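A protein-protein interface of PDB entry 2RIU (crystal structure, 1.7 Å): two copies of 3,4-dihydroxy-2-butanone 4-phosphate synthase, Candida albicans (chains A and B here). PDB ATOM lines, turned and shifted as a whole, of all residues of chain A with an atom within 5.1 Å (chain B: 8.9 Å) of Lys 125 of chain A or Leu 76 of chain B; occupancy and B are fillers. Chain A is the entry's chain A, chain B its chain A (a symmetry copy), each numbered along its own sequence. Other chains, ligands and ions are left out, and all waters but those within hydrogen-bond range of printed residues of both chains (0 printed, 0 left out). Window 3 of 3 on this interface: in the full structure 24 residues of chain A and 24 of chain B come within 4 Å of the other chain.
The side-chain hydroxyl of Thr 90 of chain A sits at hydrogen-bond distance from the side-chain sulfur of Met 75 of chain B (3.4 Å).
The backbone NH of Met 75 of chain B lies within hydrogen-bond range of the backbone carbonyl oxygen of Tyr 87 of chain B (2.8 Å).
The backbone carbonyl oxygen (O) of Glu 71 of chain A sits at hydrogen-bond distance from the side-chain amino group (NZ) of Lys 125 of chain A (3.1 Å).
The side-chain hydroxyl (OG1) of Thr 90 of chain A is in hydrogen-bond range of the backbone NH (N) of Gly 127 of chain A, 2.9 Å away.
Ile 89 of chain A touches Leu 76 of chain B.
Leu 76 of chain B touches Lys 125 of chain A (CD1 to O, 3.4 Å).
Pro 126 of chain A touches Met 75 of chain B (CB to SD, 3.9 Å).
Pro 126 of chain A touches Tyr 87 of chain B.
CE1 of Tyr 87 of chain B touches O of Gly 127 of chain A, at 3.9 Å.
Printed residues of chain B within 4 Å of Ile 89 of chain A: Leu 76.
Of the printed residues of chain B, Thr 90 of chain A touches Met 75 (3.4 Å).
Lys 125 of chain A touches just one residue of chain B: Leu 76.
Pro 126 of chain A touches two residues of chain B.
Of the printed residues of chain B, Gly 127 of chain A touches Tyr 87.
Of the printed residues of chain A, Leu 76 of chain B touches Ile 89 (3.7 Å) and Lys 125 (3.4 Å).
Printed residues of chain A within 4 Å of Tyr 87 of chain B: Pro 126 (3.7 Å) and Gly 127 (3.9 Å).
The nearest residue of chain B that does not touch Lys 125 of chain A is Met 75 of chain B (6.7 Å).
The nearest residue of chain A that does not touch Leu 76 of chain B is Pro 126 of chain A (4.3 Å).
The nearest printed residue of chain B that does not touch Thr 90 of chain A is Tyr 87 of chain B (5.1 Å).
Hydrophobic or aromatic side chains of chain A within 4 Å of the printed part of chain B: Ile 89 and Pro 126.
Along chain A the printed residues that touch a printed residue of chain B span positions 89 to 127.
Of the 10 printed residues of chain B, 3 touch a printed residue of chain A.
Along chain B the printed residues that touch a printed residue of chain A span positions 75 to 87.
Among the printed residues, no Asp or Glu carboxylate lies within 4 Å of a Lys or Arg side-chain nitrogen of the other chain.
Position printed for both chains: 89.
Of the 6 pairs that touch across the chains among the printed residues, none has its exchanged pair printed and touching as well.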
ATOM      1  N   LEU A  70     -29.527 -12.390  -9.896  1.00  0.00           N
ATOM      2  CA  LEU A  70     -28.179 -12.748 -10.347  1.00  0.00           C
ATOM      3  C   LEU A  70     -28.104 -14.127 -11.010  1.00  0.00           C
ATOM      4  O   LEU A  70     -27.027 -14.564 -11.436  1.00  0.00           O
ATOM      5  CB  LEU A  70     -27.183 -12.653  -9.185  1.00  0.00           C
ATOM      6  CG  LEU A  70     -26.844 -11.243  -8.685  1.00  0.00           C
ATOM      7  CD1 LEU A  70     -25.995 -11.305  -7.430  1.00  0.00           C
ATOM      8  CD2 LEU A  70     -26.131 -10.421  -9.764  1.00  0.00           C
ATOM      9  N   GLU A  71     -29.255 -14.795 -11.110  1.00  0.00           N
ATOM     10  CA  GLU A  71     -29.335 -16.143 -11.677  1.00  0.00           C
ATOM     11  C   GLU A  71     -28.409 -17.111 -10.941  1.00  0.00           C
ATOM     12  O   GLU A  71     -27.576 -17.795 -11.550  1.00  0.00           O
ATOM     13  CB  GLU A  71     -29.071 -16.126 -13.189  1.00  0.00           C
ATOM     14  CG  GLU A  71     -30.165 -15.425 -13.996  1.00  0.00           C
ATOM     15  CD  GLU A  71     -29.888 -15.405 -15.498  1.00  0.00           C
ATOM     16  OE1 GLU A  71     -29.109 -16.247 -15.987  1.00  0.00           O
ATOM     17  OE2 GLU A  71     -30.450 -14.533 -16.191  1.00  0.00           O
ATOM     18  N   LEU A  72     -28.565 -17.144  -9.618  1.00  0.00           N
ATOM     19  CA  LEU A  72     -27.844 -18.081  -8.762  1.00  0.00           C
ATOM     20  C   LEU A  72     -28.841 -19.041  -8.124  1.00  0.00           C
ATOM     21  O   LEU A  72     -29.287 -18.815  -6.996  1.00  0.00           O
ATOM     22  CB  LEU A  72     -27.045 -17.333  -7.687  1.00  0.00           C
ATOM     23  CG  LEU A  72     -25.906 -16.441  -8.178  1.00  0.00           C
ATOM     24  CD1 LEU A  72     -25.477 -15.492  -7.072  1.00  0.00           C
ATOM     25  CD2 LEU A  72     -24.732 -17.274  -8.684  1.00  0.00           C
ATOM     26  N   ILE A  89     -25.528 -22.446  -6.590  1.00  0.00           N
ATOM     27  CA  ILE A  89     -24.341 -22.742  -7.391  1.00  0.00           C
ATOM     28  C   ILE A  89     -23.249 -21.734  -7.007  1.00  0.00           C
ATOM     29  O   ILE A  89     -23.538 -20.555  -6.773  1.00  0.00           O
ATOM     30  CB  ILE A  89     -24.634 -22.709  -8.920  1.00  0.00           C
ATOM     31  CG1 ILE A  89     -23.407 -23.162  -9.720  1.00  0.00           C
ATOM     32  CG2 ILE A  89     -25.093 -21.316  -9.372  1.00  0.00           C
ATOM     33  CD1 ILE A  89     -23.712 -23.564 -11.147  1.00  0.00           C
ATOM     34  N   THR A  90     -22.007 -22.203  -6.912  1.00  0.00           N
ATOM     35  CA  THR A  90     -20.886 -21.328  -6.547  1.00  0.00           C
ATOM     36  C   THR A  90     -20.515 -20.409  -7.705  1.00  0.00           C
ATOM     37  O   THR A  90     -20.932 -20.641  -8.838  1.00  0.00           O
ATOM     38  CB  THR A  90     -19.658 -22.143  -6.115  1.00  0.00           C
ATOM     39  OG1 THR A  90     -19.268 -23.014  -7.185  1.00  0.00           O
ATOM     40  CG2 THR A  90     -19.980 -22.968  -4.876  1.00  0.00           C
ATOM     41  N   CYS A  91     -19.745 -19.357  -7.428  1.00  0.00           N
ATOM     42  CA  CYS A  91     -19.415 -18.397  -8.485  1.00  0.00           C
ATOM     43  C   CYS A  91     -18.157 -17.576  -8.226  1.00  0.00           C
ATOM     44  O   CYS A  91     -17.700 -17.468  -7.093  1.00  0.00           O
ATOM     45  CB  CYS A  91     -20.609 -17.462  -8.733  1.00  0.00           C
ATOM     46  SG  CYS A  91     -20.915 -16.299  -7.387  1.00  0.00           S
ATOM     47  N   PRO A 120     -26.153 -10.997 -14.092  1.00  0.00           N
ATOM     48  CA  PRO A 120     -25.895 -12.446 -14.058  1.00  0.00           C
ATOM     49  C   PRO A 120     -24.677 -12.869 -14.882  1.00  0.00           C
ATOM     50  O   PRO A 120     -23.889 -13.709 -14.437  1.00  0.00           O
ATOM     51  CB  PRO A 120     -27.161 -13.054 -14.675  1.00  0.00           C
ATOM     52  CG  PRO A 120     -28.206 -12.021 -14.542  1.00  0.00           C
ATOM     53  CD  PRO A 120     -27.551 -10.688 -14.460  1.00  0.00           C
ATOM     54  N   PHE A 123     -20.692 -13.098 -13.841  1.00  0.00           N
ATOM     55  CA  PHE A 123     -20.162 -14.161 -12.991  1.00  0.00           C
ATOM     56  C   PHE A 123     -19.915 -15.453 -13.751  1.00  0.00           C
ATOM     57  O   PHE A 123     -20.673 -15.811 -14.666  1.00  0.00           O
ATOM     58  CB  PHE A 123     -21.121 -14.440 -11.834  1.00  0.00           C
ATOM     59  CG  PHE A 123     -21.322 -13.264 -10.927  1.00  0.00           C
ATOM     60  CD1 PHE A 123     -22.315 -12.330 -11.191  1.00  0.00           C
ATOM     61  CD2 PHE A 123     -20.505 -13.080  -9.811  1.00  0.00           C
ATOM     62  CE1 PHE A 123     -22.502 -11.231 -10.360  1.00  0.00           C
ATOM     63  CE2 PHE A 123     -20.682 -11.987  -8.975  1.00  0.00           C
ATOM     64  CZ  PHE A 123     -21.681 -11.058  -9.252  1.00  0.00           C
ATOM     65  N   ILE A 124     -18.858 -16.149 -13.356  1.00  0.00           N
ATOM     66  CA  ILE A 124     -18.570 -17.490 -13.854  1.00  0.00           C
ATOM     67  C   ILE A 124     -19.081 -18.484 -12.824  1.00  0.00           C
ATOM     68  O   ILE A 124     -18.865 -18.308 -11.625  1.00  0.00           O
ATOM     69  CB  ILE A 124     -17.057 -17.720 -14.079  1.00  0.00           C
ATOM     70  CG1 ILE A 124     -16.483 -16.666 -15.034  1.00  0.00           C
ATOM     71  CG2 ILE A 124     -16.797 -19.138 -14.613  1.00  0.00           C
ATOM     72  CD1 ILE A 124     -14.974 -16.488 -14.926  1.00  0.00           C
ATOM     73  N   LYS A 125     -19.761 -19.522 -13.299  1.00  0.00           N
ATOM     74  CA  LYS A 125     -20.246 -20.591 -12.434  1.00  0.00           C
ATOM     75  C   LYS A 125     -19.810 -21.934 -13.021  1.00  0.00           C
ATOM     76  O   LYS A 125     -19.876 -22.124 -14.243  1.00  0.00           O
ATOM     77  CB  LYS A 125     -21.771 -20.527 -12.305  1.00  0.00           C
ATOM     78  CG  LYS A 125     -22.295 -19.217 -11.694  1.00  0.00           C
ATOM     79  CD  LYS A 125     -23.767 -18.990 -11.995  1.00  0.00           C
ATOM     80  CE  LYS A 125     -24.002 -18.691 -13.467  1.00  0.00           C
ATOM     81  NZ  LYS A 125     -25.346 -18.107 -13.696  1.00  0.00           N
ATOM     82  N   PRO A 126     -19.334 -22.855 -12.167  1.00  0.00           N
ATOM     83  CA  PRO A 126     -19.085 -22.696 -10.726  1.00  0.00           C
ATOM     84  C   PRO A 126     -17.874 -21.809 -10.426  1.00  0.00           C
ATOM     85  O   PRO A 126     -17.170 -21.366 -11.342  1.00  0.00           O
ATOM     86  CB  PRO A 126     -18.818 -24.132 -10.267  1.00  0.00           C
ATOM     87  CG  PRO A 126     -18.242 -24.788 -11.460  1.00  0.00           C
ATOM     88  CD  PRO A 126     -19.021 -24.226 -12.615  1.00  0.00           C
ATOM     89  N   GLY A 127     -17.638 -21.553  -9.145  1.00  0.00           N
ATOM     90  CA  GLY A 127     -16.531 -20.702  -8.741  1.00  0.00           C
ATOM     91  C   GLY A 127     -16.059 -21.000  -7.340  1.00  0.00           C
ATOM     92  O   GLY A 127     -16.138 -22.138  -6.883  1.00  0.00           O
ATOM     93  N   PRO B  73     -23.115 -35.586  -9.351  1.00  0.00           N
ATOM     94  CA  PRO B  73     -23.075 -35.005 -10.683  1.00  0.00           C
ATOM     95  C   PRO B  73     -22.331 -33.678 -10.684  1.00  0.00           C
ATOM     96  O   PRO B  73     -22.220 -33.045  -9.632  1.00  0.00           O
ATOM     97  CB  PRO B  73     -24.557 -34.789 -11.021  1.00  0.00           C
ATOM     98  CG  PRO B  73     -25.248 -34.690  -9.731  1.00  0.00           C
ATOM     99  CD  PRO B  73     -24.452 -35.483  -8.739  1.00  0.00           C
ATOM    100  N   PRO B  74     -21.825 -33.251 -11.856  1.00  0.00           N
ATOM    101  CA  PRO B  74     -21.216 -31.925 -11.948  1.00  0.00           C
ATOM    102  C   PRO B  74     -22.153 -30.869 -11.374  1.00  0.00           C
ATOM    103  O   PRO B  74     -23.373 -30.965 -11.523  1.00  0.00           O
ATOM    104  CB  PRO B  74     -21.058 -31.724 -13.459  1.00  0.00           C
ATOM    105  CG  PRO B  74     -20.900 -33.094 -13.992  1.00  0.00           C
ATOM    106  CD  PRO B  74     -21.799 -33.954 -13.153  1.00  0.00           C
ATOM    107  N   MET B  75     -21.588 -29.876 -10.697  1.00  0.00           N
ATOM    108  CA  MET B  75     -22.407 -28.849 -10.076  1.00  0.00           C
ATOM    109  C   MET B  75     -23.224 -28.120 -11.135  1.00  0.00           C
ATOM    110  O   MET B  75     -24.394 -27.791 -10.907  1.00  0.00           O
ATOM    111  CB  MET B  75     -21.534 -27.873  -9.307  1.00  0.00           C
ATOM    112  CG  MET B  75     -22.305 -26.980  -8.374  1.00  0.00           C
ATOM    113  SD  MET B  75     -21.184 -25.784  -7.655  1.00  0.00           S
ATOM    114  CE  MET B  75     -20.365 -26.767  -6.390  1.00  0.00           C
ATOM    115  N   LEU B  76     -22.592 -27.871 -12.282  1.00  0.00           N
ATOM    116  CA  LEU B  76     -23.272 -27.360 -13.468  1.00  0.00           C
ATOM    117  C   LEU B  76     -23.068 -28.361 -14.600  1.00  0.00           C
ATOM    118  O   LEU B  76     -21.929 -28.624 -15.003  1.00  0.00           O
ATOM    119  CB  LEU B  76     -22.704 -25.997 -13.870  1.00  0.00           C
ATOM    120  CG  LEU B  76     -23.613 -24.948 -14.525  1.00  0.00           C
ATOM    121  CD1 LEU B  76     -22.827 -23.655 -14.731  1.00  0.00           C
ATOM    122  CD2 LEU B  76     -24.248 -25.409 -15.837  1.00  0.00           C
ATOM    123  N   THR B  85     -11.852 -26.369 -13.226  1.00  0.00           N
ATOM    124  CA  THR B  85     -12.023 -27.312 -12.119  1.00  0.00           C
ATOM    125  C   THR B  85     -13.437 -27.911 -12.150  1.00  0.00           C
ATOM    126  O   THR B  85     -14.428 -27.181 -12.237  1.00  0.00           O
ATOM    127  CB  THR B  85     -11.760 -26.625 -10.762  1.00  0.00           C
ATOM    128  OG1 THR B  85     -10.478 -25.982 -10.787  1.00  0.00           O
ATOM    129  CG2 THR B  85     -11.802 -27.632  -9.615  1.00  0.00           C
ATOM    130  N   ALA B  86     -13.516 -29.237 -12.080  1.00  0.00           N
ATOM    131  CA  ALA B  86     -14.778 -29.945 -12.269  1.00  0.00           C
ATOM    132  C   ALA B  86     -15.494 -30.251 -10.953  1.00  0.00           C
ATOM    133  O   ALA B  86     -15.520 -31.397 -10.502  1.00  0.00           O
ATOM    134  CB  ALA B  86     -14.547 -31.229 -13.080  1.00  0.00           C
ATOM    135  N   TYR B  87     -16.078 -29.219 -10.345  1.00  0.00           N
ATOM    136  CA  TYR B  87     -16.819 -29.380  -9.096  1.00  0.00           C
ATOM    137  C   TYR B  87     -18.082 -30.208  -9.287  1.00  0.00           C
ATOM    138  O   TYR B  87     -18.807 -30.029 -10.272  1.00  0.00           O
ATOM    139  CB  TYR B  87     -17.222 -28.013  -8.532  1.00  0.00           C
ATOM    140  CG  TYR B  87     -16.069 -27.107  -8.216  1.00  0.00           C
ATOM    141  CD1 TYR B  87     -15.704 -26.084  -9.094  1.00  0.00           C
ATOM    142  CD2 TYR B  87     -15.334 -27.265  -7.038  1.00  0.00           C
ATOM    143  CE1 TYR B  87     -14.635 -25.242  -8.807  1.00  0.00           C
ATOM    144  CE2 TYR B  87     -14.257 -26.431  -6.744  1.00  0.00           C
ATOM    145  CZ  TYR B  87     -13.920 -25.419  -7.634  1.00  0.00           C
ATOM    146  OH  TYR B  87     -12.863 -24.593  -7.346  1.00  0.00           O
ATOM    147  N   THR B  88     -18.333 -31.112  -8.345  1.00  0.00           N
ATOM    148  CA  THR B  88     -19.620 -31.793  -8.253  1.00  0.00           C
ATOM    149  C   THR B  88     -20.493 -31.034  -7.256  1.00  0.00           C
ATOM    150  O   THR B  88     -20.021 -30.097  -6.597  1.00  0.00           O
ATOM    151  CB  THR B  88     -19.481 -33.271  -7.792  1.00  0.00           C
ATOM    152  OG1 THR B  88     -19.240 -33.335  -6.378  1.00  0.00           O
ATOM    153  CG2 THR B  88     -18.366 -33.985  -8.544  1.00  0.00           C
ATOM    154  N   ILE B  89     -21.762 -31.426  -7.143  1.00  0.00           N
ATOM    155  CA  ILE B  89     -22.568 -30.991  -6.004  1.00  0.00           C
ATOM    156  C   ILE B  89     -21.789 -31.317  -4.722  1.00  0.00           C
ATOM    157  O   ILE B  89     -21.137 -32.364  -4.633  1.00  0.00           O
ATOM    158  CB  ILE B  89     -23.981 -31.646  -5.993  1.00  0.00           C
ATOM    159  CG1 ILE B  89     -24.844 -31.061  -4.869  1.00  0.00           C
ATOM    160  CG2 ILE B  89     -23.889 -33.173  -5.868  1.00  0.00           C
ATOM    161  CD1 ILE B  89     -26.328 -31.311  -5.034  1.00  0.00           C
ATOM    162  N   ARG B 133     -14.182 -34.019 -10.104  1.00  0.00           N
ATOM    163  CA  ARG B 133     -14.150 -35.132 -11.048  1.00  0.00           C
ATOM    164  C   ARG B 133     -12.883 -35.091 -11.904  1.00  0.00           C
ATOM    165  O   ARG B 133     -12.749 -34.239 -12.791  1.00  0.00           O
ATOM    166  CB  ARG B 133     -15.392 -35.095 -11.942  1.00  0.00           C
ATOM    167  CG  ARG B 133     -16.643 -35.671 -11.304  1.00  0.00           C
ATOM    168  CD  ARG B 133     -17.941 -35.181 -11.982  1.00  0.00           C
ATOM    169  NE  ARG B 133     -19.110 -35.933 -11.522  1.00  0.00           N
ATOM    170  CZ  ARG B 133     -19.510 -37.098 -12.030  1.00  0.00           C
ATOM    171  NH1 ARG B 133     -18.838 -37.672 -13.014  1.00  0.00           N
ATOM    172  NH2 ARG B 133     -20.587 -37.698 -11.544  1.00  0.00           N
